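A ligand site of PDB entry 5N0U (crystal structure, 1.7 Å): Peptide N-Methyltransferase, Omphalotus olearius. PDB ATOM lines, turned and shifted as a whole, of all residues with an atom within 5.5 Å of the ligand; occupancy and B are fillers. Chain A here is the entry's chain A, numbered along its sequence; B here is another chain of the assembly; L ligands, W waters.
The side-chain sulfur of Met 214 is in hydrogen-bond range of a nitrogen (N4) of the ligand (3.5 Å).
A nitrogen (N1) of the ligand is in hydrogen-bond range of the backbone carbonyl oxygen of Val 102.
O5 of the ligand lies within hydrogen-bond range of O of Ser 243 (3.0 Å).
The backbone carbonyl oxygen of His 99 lies within hydrogen-bond range of a nitrogen (N1) of the ligand, at 3.0 Å.
The side-chain amide oxygen of Gln 171 sits close to an oxygen (O4) of the ligand.
N of His 99 lies within hydrogen-bond range of O2 of the ligand.
The side-chain hydroxyl of Tyr 97 lies within hydrogen-bond range of a nitrogen (N3) of the ligand, 2.7 Å away.
O of Tyr 97 sits at hydrogen-bond distance from N1 of the ligand.
N of Ala 129 sits at hydrogen-bond distance from O1 of the ligand, 2.9 Å away.
N of Ala 212 lies within hydrogen-bond range of N5 of the ligand (2.8 Å).
An oxygen (O5) of the ligand lies within hydrogen-bond range of the backbone NH of Gln 171, at 2.9 Å.
A nitrogen (N4) of the ligand sits at hydrogen-bond distance from the backbone carbonyl oxygen (O) of Ala 212.
The side-chain hydroxyl of Thr 244 sits at hydrogen-bond distance from a nitrogen (N6) of the ligand (2.7 Å).
An oxygen (O4) of the ligand is in hydrogen-bond range of the backbone carbonyl oxygen of Gly 241, at 3.2 Å.
O of Thr 244 sits at hydrogen-bond distance from N of Tyr 210 (2.8 Å).
The side-chain sulfur (SG) of Cys 174 sits at hydrogen-bond distance from the side-chain amide oxygen (OE1) of Gln 171 (3.0 Å).
The backbone NH of Gly 240 lies within hydrogen-bond range of the side-chain hydroxyl of Ser 243, at 2.9 Å.
The side-chain hydroxyl (OH) of Tyr 97 is in hydrogen-bond range of the side-chain sulfur (SD) of Met 214, 3.6 Å away.
N of Glu 130 lies close to OG of Ser 128 (3.2 Å).
The backbone carbonyl oxygen (O) of Val 127 lies within hydrogen-bond range of the backbone NH (N) of His 99, at 3.4 Å.
A nitrogen (N6) of the ligand lies close to the backbone carbonyl oxygen of Val 242 (3.1 Å).
CG2 of Ile 18 touches N4 of the ligand, at 3.7 Å.
CA of Gly 98 touches O2 of the ligand, 3.6 Å away.
Phe 103 touches the ligand (CB to S1, 3.5 Å).
CG2 of Val 104 touches N1 of the ligand, 3.7 Å away.
Ser 128 touches the ligand (CA to O2, 3.4 Å).
Phe 170 touches the ligand (CA to O5, 3.2 Å).
Tyr 210 touches the ligand (O to C13, 3.5 Å).
CA of Ile 211 touches N5 of the ligand, 3.5 Å away.
Ile 401 of chain B touches the ligand (CD1 to C5, 3.8 Å).
Hydrophobic or aromatic side chains that line the ligand: Ile 18, Tyr 97, His 99, Val 102, Phe 103, Val 104, Ala 129, Phe 170, Tyr 210, Ala 212, Met 214, Val 242 and Ile 401 of chain B.
20 residues have an atom within 4 Å of the ligand: Ile 18, Tyr 97, Gly 98, His 99, Val 102, Phe 103, Val 104, Ser 128, Ala 129, Phe 170, Gln 171, Tyr 210, Ile 211, Ala 212, Met 214, Gly 241, Val 242, Ser 243, Thr 244 and Ile 401 of chain B.
The nearest printed residue that does not touch the ligand is Val 127 (4.4 Å).
Water W2 bridges O of Tyr 97 and N1 of the ligand.
Water W1 lies within hydrogen-bond range of the backbone carbonyl oxygen of Ser 243, the backbone carbonyl oxygen of Gly 240, an oxygen (O4) of the ligand and the backbone NH of Val 172.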
ATOM      1  N   ILE A  18      -1.707 -27.021   7.847  1.00  0.00           N
ATOM      2  CA  ILE A  18      -0.954 -25.811   8.124  1.00  0.00           C
ATOM      3  C   ILE A  18      -1.369 -24.692   7.168  1.00  0.00           C
ATOM      4  O   ILE A  18      -1.706 -23.588   7.593  1.00  0.00           O
ATOM      5  CB  ILE A  18       0.560 -26.100   8.035  1.00  0.00           C
ATOM      6  CG1 ILE A  18       0.979 -27.123   9.103  1.00  0.00           C
ATOM      7  CG2 ILE A  18       1.403 -24.835   8.133  1.00  0.00           C
ATOM      8  CD1 ILE A  18       0.816 -26.671  10.552  1.00  0.00           C
ATOM      9  N   ILE A  43      -5.232 -20.560  13.351  1.00  0.00           N
ATOM     10  CA  ILE A  43      -4.408 -19.355  13.435  1.00  0.00           C
ATOM     11  C   ILE A  43      -4.512 -18.403  12.257  1.00  0.00           C
ATOM     12  O   ILE A  43      -3.773 -17.412  12.207  1.00  0.00           O
ATOM     13  CB  ILE A  43      -2.932 -19.657  13.807  1.00  0.00           C
ATOM     14  CG1 ILE A  43      -2.211 -20.398  12.694  1.00  0.00           C
ATOM     15  CG2 ILE A  43      -2.867 -20.461  15.094  1.00  0.00           C
ATOM     16  CD1 ILE A  43      -0.724 -20.525  12.973  1.00  0.00           C
ATOM     17  N   TYR A  97      -5.379 -26.466  14.475  1.00  0.00           N
ATOM     18  CA  TYR A  97      -4.341 -26.209  13.468  1.00  0.00           C
ATOM     19  C   TYR A  97      -3.416 -27.400  13.286  1.00  0.00           C
ATOM     20  O   TYR A  97      -2.982 -28.020  14.257  1.00  0.00           O
ATOM     21  CB  TYR A  97      -3.555 -24.983  13.933  1.00  0.00           C
ATOM     22  CG  TYR A  97      -2.381 -24.521  13.128  1.00  0.00           C
ATOM     23  CD1 TYR A  97      -2.545 -24.024  11.827  1.00  0.00           C
ATOM     24  CD2 TYR A  97      -1.109 -24.464  13.695  1.00  0.00           C
ATOM     25  CE1 TYR A  97      -1.463 -23.541  11.101  1.00  0.00           C
ATOM     26  CE2 TYR A  97      -0.023 -23.991  12.979  1.00  0.00           C
ATOM     27  CZ  TYR A  97      -0.192 -23.539  11.685  1.00  0.00           C
ATOM     28  OH  TYR A  97       0.896 -23.023  11.003  1.00  0.00           O
ATOM     29  N   GLY A  98      -3.117 -27.722  12.044  1.00  0.00           N
ATOM     30  CA  GLY A  98      -2.146 -28.763  11.736  1.00  0.00           C
ATOM     31  C   GLY A  98      -2.729 -30.136  11.949  1.00  0.00           C
ATOM     32  O   GLY A  98      -3.838 -30.415  11.489  1.00  0.00           O
ATOM     33  N   HIS A  99      -1.934 -31.003  12.582  1.00  0.00           N
ATOM     34  CA  HIS A  99      -2.376 -32.293  13.109  1.00  0.00           C
ATOM     35  C   HIS A  99      -2.844 -31.989  14.535  1.00  0.00           C
ATOM     36  O   HIS A  99      -2.082 -31.439  15.322  1.00  0.00           O
ATOM     37  CB  HIS A  99      -1.201 -33.257  13.130  1.00  0.00           C
ATOM     38  CG  HIS A  99      -1.518 -34.659  13.543  1.00  0.00           C
ATOM     39  ND1 HIS A  99      -2.145 -34.975  14.737  1.00  0.00           N
ATOM     40  CD2 HIS A  99      -1.160 -35.844  12.991  1.00  0.00           C
ATOM     41  CE1 HIS A  99      -2.208 -36.287  14.862  1.00  0.00           C
ATOM     42  NE2 HIS A  99      -1.613 -36.834  13.824  1.00  0.00           N
ATOM     43  N   PRO A 100      -4.068 -32.379  14.890  1.00  0.00           N
ATOM     44  CA  PRO A 100      -4.630 -31.954  16.170  1.00  0.00           C
ATOM     45  C   PRO A 100      -4.075 -32.655  17.415  1.00  0.00           C
ATOM     46  O   PRO A 100      -4.485 -32.305  18.536  1.00  0.00           O
ATOM     47  CB  PRO A 100      -6.106 -32.271  15.990  1.00  0.00           C
ATOM     48  CG  PRO A 100      -6.084 -33.521  15.152  1.00  0.00           C
ATOM     49  CD  PRO A 100      -5.021 -33.230  14.141  1.00  0.00           C
ATOM     50  N   VAL A 102      -0.506 -33.105  17.610  1.00  0.00           N
ATOM     51  CA  VAL A 102       0.924 -32.780  17.537  1.00  0.00           C
ATOM     52  C   VAL A 102       1.125 -31.452  18.245  1.00  0.00           C
ATOM     53  O   VAL A 102       0.703 -30.402  17.755  1.00  0.00           O
ATOM     54  CB  VAL A 102       1.388 -32.754  16.049  1.00  0.00           C
ATOM     55  CG1 VAL A 102       2.783 -32.161  15.859  1.00  0.00           C
ATOM     56  CG2 VAL A 102       1.351 -34.149  15.474  1.00  0.00           C
ATOM     57  N   PHE A 103       1.756 -31.501  19.423  1.00  0.00           N
ATOM     58  CA  PHE A 103       1.939 -30.344  20.298  1.00  0.00           C
ATOM     59  C   PHE A 103       0.592 -29.674  20.638  1.00  0.00           C
ATOM     60  O   PHE A 103       0.475 -28.455  20.567  1.00  0.00           O
ATOM     61  CB  PHE A 103       2.919 -29.308  19.670  1.00  0.00           C
ATOM     62  CG  PHE A 103       4.303 -29.852  19.366  1.00  0.00           C
ATOM     63  CD1 PHE A 103       4.496 -30.849  18.425  1.00  0.00           C
ATOM     64  CD2 PHE A 103       5.422 -29.358  20.022  1.00  0.00           C
ATOM     65  CE1 PHE A 103       5.752 -31.367  18.143  1.00  0.00           C
ATOM     66  CE2 PHE A 103       6.680 -29.863  19.744  1.00  0.00           C
ATOM     67  CZ  PHE A 103       6.847 -30.874  18.817  1.00  0.00           C
ATOM     68  N   VAL A 104      -0.425 -30.478  20.962  1.00  0.00           N
ATOM     69  CA  VAL A 104      -1.753 -29.953  21.342  1.00  0.00           C
ATOM     70  C   VAL A 104      -2.176 -30.720  22.575  1.00  0.00           C
ATOM     71  O   VAL A 104      -2.297 -31.935  22.505  1.00  0.00           O
ATOM     72  CB  VAL A 104      -2.816 -30.164  20.219  1.00  0.00           C
ATOM     73  CG1 VAL A 104      -4.178 -29.618  20.624  1.00  0.00           C
ATOM     74  CG2 VAL A 104      -2.362 -29.530  18.918  1.00  0.00           C
ATOM     75  N   VAL A 127      -2.286 -32.899   8.531  1.00  0.00           N
ATOM     76  CA  VAL A 127      -0.981 -32.492   8.036  1.00  0.00           C
ATOM     77  C   VAL A 127      -0.320 -31.607   9.093  1.00  0.00           C
ATOM     78  O   VAL A 127      -0.839 -30.550   9.439  1.00  0.00           O
ATOM     79  CB  VAL A 127      -1.107 -31.736   6.709  1.00  0.00           C
ATOM     80  CG1 VAL A 127       0.198 -31.041   6.321  1.00  0.00           C
ATOM     81  CG2 VAL A 127      -1.575 -32.672   5.611  1.00  0.00           C
ATOM     82  N   SER A 128       0.835 -32.046   9.589  1.00  0.00           N
ATOM     83  CA  SER A 128       1.595 -31.294  10.604  1.00  0.00           C
ATOM     84  C   SER A 128       2.628 -30.352  10.004  1.00  0.00           C
ATOM     85  O   SER A 128       2.930 -30.415   8.814  1.00  0.00           O
ATOM     86  CB  SER A 128       2.299 -32.272  11.527  1.00  0.00           C
ATOM     87  OG  SER A 128       3.400 -32.881  10.852  1.00  0.00           O
ATOM     88  N   ALA A 129       3.223 -29.507  10.838  1.00  0.00           N
ATOM     89  CA  ALA A 129       4.327 -28.669  10.390  1.00  0.00           C
ATOM     90  C   ALA A 129       5.520 -29.517   9.927  1.00  0.00           C
ATOM     91  O   ALA A 129       6.237 -29.115   8.995  1.00  0.00           O
ATOM     92  CB  ALA A 129       4.760 -27.704  11.478  1.00  0.00           C
ATOM     93  N   GLU A 130       5.718 -30.682  10.550  1.00  0.00           N
ATOM     94  CA  GLU A 130       6.795 -31.573  10.140  1.00  0.00           C
ATOM     95  C   GLU A 130       6.526 -32.160   8.742  1.00  0.00           C
ATOM     96  O   GLU A 130       7.437 -32.255   7.920  1.00  0.00           O
ATOM     97  CB  GLU A 130       7.039 -32.684  11.180  1.00  0.00           C
ATOM     98  CG  GLU A 130       8.304 -33.473  10.861  1.00  0.00           C
ATOM     99  CD  GLU A 130       8.710 -34.497  11.912  1.00  0.00           C
ATOM    100  OE1 GLU A 130       9.896 -34.507  12.257  1.00  0.00           O
ATOM    101  OE2 GLU A 130       7.902 -35.306  12.365  1.00  0.00           O
ATOM    102  N   LEU A 169      13.385 -29.407  15.256  1.00  0.00           N
ATOM    103  CA  LEU A 169      13.058 -28.749  16.515  1.00  0.00           C
ATOM    104  C   LEU A 169      11.882 -27.792  16.338  1.00  0.00           C
ATOM    105  O   LEU A 169      11.986 -26.811  15.596  1.00  0.00           O
ATOM    106  CB  LEU A 169      14.269 -27.980  17.046  1.00  0.00           C
ATOM    107  CG  LEU A 169      15.499 -28.821  17.382  1.00  0.00           C
ATOM    108  CD1 LEU A 169      16.647 -27.923  17.839  1.00  0.00           C
ATOM    109  CD2 LEU A 169      15.208 -29.873  18.451  1.00  0.00           C
ATOM    110  N   PHE A 170      10.785 -28.089  17.033  1.00  0.00           N
ATOM    111  CA  PHE A 170       9.574 -27.238  17.098  1.00  0.00           C
ATOM    112  C   PHE A 170       9.756 -26.174  18.206  1.00  0.00           C
ATOM    113  O   PHE A 170      10.539 -26.376  19.152  1.00  0.00           O
ATOM    114  CB  PHE A 170       8.337 -28.057  17.478  1.00  0.00           C
ATOM    115  CG  PHE A 170       7.683 -28.840  16.357  1.00  0.00           C
ATOM    116  CD1 PHE A 170       8.327 -29.912  15.766  1.00  0.00           C
ATOM    117  CD2 PHE A 170       6.352 -28.572  15.990  1.00  0.00           C
ATOM    118  CE1 PHE A 170       7.701 -30.652  14.756  1.00  0.00           C
ATOM    119  CE2 PHE A 170       5.707 -29.306  14.995  1.00  0.00           C
ATOM    120  CZ  PHE A 170       6.388 -30.353  14.372  1.00  0.00           C
ATOM    121  N   GLN A 171       9.012 -25.067  18.101  1.00  0.00           N
ATOM    122  CA  GLN A 171       8.922 -24.063  19.172  1.00  0.00           C
ATOM    123  C   GLN A 171      10.285 -23.431  19.498  1.00  0.00           C
ATOM    124  O   GLN A 171      10.585 -23.111  20.652  1.00  0.00           O
ATOM    125  CB  GLN A 171       8.238 -24.639  20.441  1.00  0.00           C
ATOM    126  CG  GLN A 171       6.787 -25.086  20.240  1.00  0.00           C
ATOM    127  CD  GLN A 171       5.763 -23.960  20.380  1.00  0.00           C
ATOM    128  OE1 GLN A 171       6.113 -22.774  20.419  1.00  0.00           O
ATOM    129  NE2 GLN A 171       4.483 -24.331  20.443  1.00  0.00           N
ATOM    130  N   VAL A 172      11.096 -23.234  18.459  1.00  0.00           N
ATOM    131  CA  VAL A 172      12.397 -22.582  18.584  1.00  0.00           C
ATOM    132  C   VAL A 172      12.271 -21.072  18.829  1.00  0.00           C
ATOM    133  O   VAL A 172      13.217 -20.445  19.296  1.00  0.00           O
ATOM    134  CB  VAL A 172      13.337 -22.860  17.383  1.00  0.00           C
ATOM    135  CG1 VAL A 172      13.729 -24.329  17.349  1.00  0.00           C
ATOM    136  CG2 VAL A 172      12.735 -22.433  16.053  1.00  0.00           C
ATOM    137  N   CYS A 174      10.124 -19.910  21.073  1.00  0.00           N
ATOM    138  CA  CYS A 174       9.483 -19.848  22.379  1.00  0.00           C
ATOM    139  C   CYS A 174      10.310 -20.543  23.464  1.00  0.00           C
ATOM    140  O   CYS A 174       9.756 -21.197  24.353  1.00  0.00           O
ATOM    141  CB  CYS A 174       8.103 -20.502  22.304  1.00  0.00           C
ATOM    142  SG  CYS A 174       7.106 -19.965  20.899  1.00  0.00           S
ATOM    143  N   TYR A 210      12.914 -22.757   9.033  1.00  0.00           N
ATOM    144  CA  TYR A 210      11.771 -23.162   8.203  1.00  0.00           C
ATOM    145  C   TYR A 210      10.460 -22.567   8.684  1.00  0.00           C
ATOM    146  O   TYR A 210      10.082 -22.739   9.853  1.00  0.00           O
ATOM    147  CB  TYR A 210      11.650 -24.688   8.151  1.00  0.00           C
ATOM    148  CG  TYR A 210      10.435 -25.135   7.379  1.00  0.00           C
ATOM    149  CD1 TYR A 210      10.323 -24.842   6.021  1.00  0.00           C
ATOM    150  CD2 TYR A 210       9.393 -25.802   7.999  1.00  0.00           C
ATOM    151  CE1 TYR A 210       9.185 -25.225   5.310  1.00  0.00           C
ATOM    152  CE2 TYR A 210       8.267 -26.180   7.289  1.00  0.00           C
ATOM    153  CZ  TYR A 210       8.175 -25.901   5.950  1.00  0.00           C
ATOM    154  OH  TYR A 210       7.053 -26.252   5.247  1.00  0.00           O
ATOM    155  N   ILE A 211       9.747 -21.899   7.774  1.00  0.00           N
ATOM    156  CA  ILE A 211       8.359 -21.478   8.011  1.00  0.00           C
ATOM    157  C   ILE A 211       7.539 -21.847   6.777  1.00  0.00           C
ATOM    158  O   ILE A 211       7.746 -21.284   5.685  1.00  0.00           O
ATOM    159  CB  ILE A 211       8.212 -19.964   8.311  1.00  0.00           C
ATOM    160  CG1 ILE A 211       9.081 -19.542   9.510  1.00  0.00           C
ATOM    161  CG2 ILE A 211       6.740 -19.643   8.580  1.00  0.00           C
ATOM    162  CD1 ILE A 211       9.155 -18.042   9.723  1.00  0.00           C
ATOM    163  N   ALA A 212       6.621 -22.802   6.954  1.00  0.00           N
ATOM    164  CA  ALA A 212       5.692 -23.201   5.900  1.00  0.00           C
ATOM    165  C   ALA A 212       4.801 -22.013   5.563  1.00  0.00           C
ATOM    166  O   ALA A 212       4.382 -21.291   6.455  1.00  0.00           O
ATOM    167  CB  ALA A 212       4.814 -24.358   6.371  1.00  0.00           C
ATOM    168  N   ALA A 213       4.506 -21.845   4.269  1.00  0.00           N
ATOM    169  CA  ALA A 213       3.509 -20.882   3.826  1.00  0.00           C
ATOM    170  C   ALA A 213       2.183 -21.184   4.538  1.00  0.00           C
ATOM    171  O   ALA A 213       1.722 -22.325   4.579  1.00  0.00           O
ATOM    172  CB  ALA A 213       3.314 -20.967   2.317  1.00  0.00           C
ATOM    173  N   MET A 214       1.595 -20.154   5.118  1.00  0.00           N
ATOM    174  CA  MET A 214       0.290 -20.289   5.733  1.00  0.00           C
ATOM    175  C   MET A 214      -0.852 -19.824   4.821  1.00  0.00           C
ATOM    176  O   MET A 214      -1.967 -20.307   4.959  1.00  0.00           O
ATOM    177  CB  MET A 214       0.276 -19.651   7.123  1.00  0.00           C
ATOM    178  CG  MET A 214       0.909 -20.589   8.158  1.00  0.00           C
ATOM    179  SD  MET A 214       1.642 -19.798   9.600  1.00  0.00           S
ATOM    180  CE  MET A 214       0.253 -18.858  10.204  1.00  0.00           C
ATOM    181  N   GLY A 240      10.394 -16.826  15.098  1.00  0.00           N
ATOM    182  CA  GLY A 240       9.138 -16.507  15.777  1.00  0.00           C
ATOM    183  C   GLY A 240       8.311 -17.727  16.118  1.00  0.00           C
ATOM    184  O   GLY A 240       8.801 -18.861  16.074  1.00  0.00           O
ATOM    185  N   GLY A 241       7.045 -17.502  16.440  1.00  0.00           N
ATOM    186  CA  GLY A 241       6.156 -18.548  16.939  1.00  0.00           C
ATOM    187  C   GLY A 241       5.775 -19.654  15.957  1.00  0.00           C
ATOM    188  O   GLY A 241       5.276 -20.698  16.374  1.00  0.00           O
ATOM    189  N   VAL A 242       5.968 -19.422  14.664  1.00  0.00           N
ATOM    190  CA  VAL A 242       5.719 -20.472  13.651  1.00  0.00           C
ATOM    191  C   VAL A 242       7.034 -20.994  13.022  1.00  0.00           C
ATOM    192  O   VAL A 242       7.007 -21.631  11.949  1.00  0.00           O
ATOM    193  CB  VAL A 242       4.702 -20.018  12.572  1.00  0.00           C
ATOM    194  CG1 VAL A 242       3.319 -19.879  13.180  1.00  0.00           C
ATOM    195  CG2 VAL A 242       5.134 -18.732  11.883  1.00  0.00           C
ATOM    196  N   SER A 243       8.158 -20.753  13.692  1.00  0.00           N
ATOM    197  CA  SER A 243       9.463 -21.164  13.186  1.00  0.00           C
ATOM    198  C   SER A 243       9.787 -22.565  13.658  1.00  0.00           C
ATOM    199  O   SER A 243       9.536 -22.925  14.814  1.00  0.00           O
ATOM    200  CB  SER A 243      10.560 -20.200  13.637  1.00  0.00           C
ATOM    201  OG  SER A 243      10.361 -18.900  13.094  1.00  0.00           O
ATOM    202  N   THR A 244      10.354 -23.360  12.750  1.00  0.00           N
ATOM    203  CA  THR A 244      10.872 -24.680  13.065  1.00  0.00           C
ATOM    204  C   THR A 244      12.296 -24.716  12.552  1.00  0.00           C
ATOM    205  O   THR A 244      12.589 -24.079  11.529  1.00  0.00           O
ATOM    206  CB  THR A 244      10.013 -25.771  12.409  1.00  0.00           C
ATOM    207  OG1 THR A 244       8.704 -25.725  12.975  1.00  0.00           O
ATOM    208  CG2 THR A 244      10.602 -27.168  12.613  1.00  0.00           C
ATOM    209  N   ILE B 401       1.505 -19.857  19.196  1.00  0.00           N
ATOM    210  CA  ILE B 401       0.440 -20.871  19.291  1.00  0.00           C
ATOM    211  C   ILE B 401       0.168 -21.202  20.764  1.00  0.00           C
ATOM    212  O   ILE B 401      -0.837 -20.744  21.315  1.00  0.00           O
ATOM    213  CB  ILE B 401       0.748 -22.137  18.435  1.00  0.00           C
ATOM    214  CG1 ILE B 401       0.812 -21.781  16.939  1.00  0.00           C
ATOM    215  CG2 ILE B 401      -0.324 -23.212  18.670  1.00  0.00           C
ATOM    216  CD1 ILE B 401       2.146 -21.265  16.464  1.00  0.00           C
ATOM    217  N   VAL B 403      -0.619 -24.258  22.364  1.00  0.00           N
ATOM    218  CA  VAL B 403      -1.779 -25.121  22.582  1.00  0.00           C
ATOM    219  C   VAL B 403      -1.330 -26.489  23.160  1.00  0.00           C
ATOM    220  O   VAL B 403      -2.148 -27.383  23.302  1.00  0.00           O
ATOM    221  CB  VAL B 403      -2.623 -25.219  21.273  1.00  0.00           C
ATOM    222  CG1 VAL B 403      -1.930 -26.066  20.218  1.00  0.00           C
ATOM    223  CG2 VAL B 403      -4.053 -25.690  21.553  1.00  0.00           C
HETATM  224  N1  LIG L   1      -0.406 -29.006  15.804  1.00  0.00           N
HETATM  225  C1  LIG L   1       0.615 -28.249  15.064  1.00  0.00           C
HETATM  226  C2  LIG L   1       1.743 -27.770  15.989  1.00  0.00           C
HETATM  227  C3  LIG L   1       1.302 -26.832  17.089  1.00  0.00           C
HETATM  228  S1  LIG L   1       2.675 -26.192  18.042  1.00  0.00           S
HETATM  229  C4  LIG L   1       1.198 -29.106  13.986  1.00  0.00           C
HETATM  230  O1  LIG L   1       2.290 -28.828  13.465  1.00  0.00           O
HETATM  231  O2  LIG L   1       0.605 -30.108  13.583  1.00  0.00           O
HETATM  232  C5  LIG L   1       3.278 -24.900  17.005  1.00  0.00           C
HETATM  233  C6  LIG L   1       4.713 -25.224  16.523  1.00  0.00           C
HETATM  234  O3  LIG L   1       4.627 -25.944  15.277  1.00  0.00           O
HETATM  235  C7  LIG L   1       5.589 -24.014  16.196  1.00  0.00           C
HETATM  236  O4  LIG L   1       6.361 -23.528  17.305  1.00  0.00           O
HETATM  237  C8  LIG L   1       6.494 -24.498  15.076  1.00  0.00           C
HETATM  238  O5  LIG L   1       7.663 -25.188  15.575  1.00  0.00           O
HETATM  239  C9  LIG L   1       5.574 -25.462  14.322  1.00  0.00           C
HETATM  240  N2  LIG L   1       4.876 -24.696  13.275  1.00  0.00           N
HETATM  241  C10 LIG L   1       3.636 -24.173  13.320  1.00  0.00           C
HETATM  242  N3  LIG L   1       3.336 -23.526  12.167  1.00  0.00           N
HETATM  243  C11 LIG L   1       4.421 -23.621  11.376  1.00  0.00           C
HETATM  244  C12 LIG L   1       4.802 -23.153  10.041  1.00  0.00           C
HETATM  245  N4  LIG L   1       3.905 -22.431   9.334  1.00  0.00           N
HETATM  246  N5  LIG L   1       6.011 -23.487   9.568  1.00  0.00           N
HETATM  247  C13 LIG L   1       6.904 -24.222  10.296  1.00  0.00           C
HETATM  248  N6  LIG L   1       6.632 -24.661  11.546  1.00  0.00           N
HETATM  249  C14 LIG L   1       5.425 -24.398  12.102  1.00  0.00           C
HETATM  250  O   HOH W   1       8.779 -21.572  17.048  1.00  0.00           O
HETATM  251  O   HOH W   2      -2.185 -27.032  16.691  1.00  0.00           O
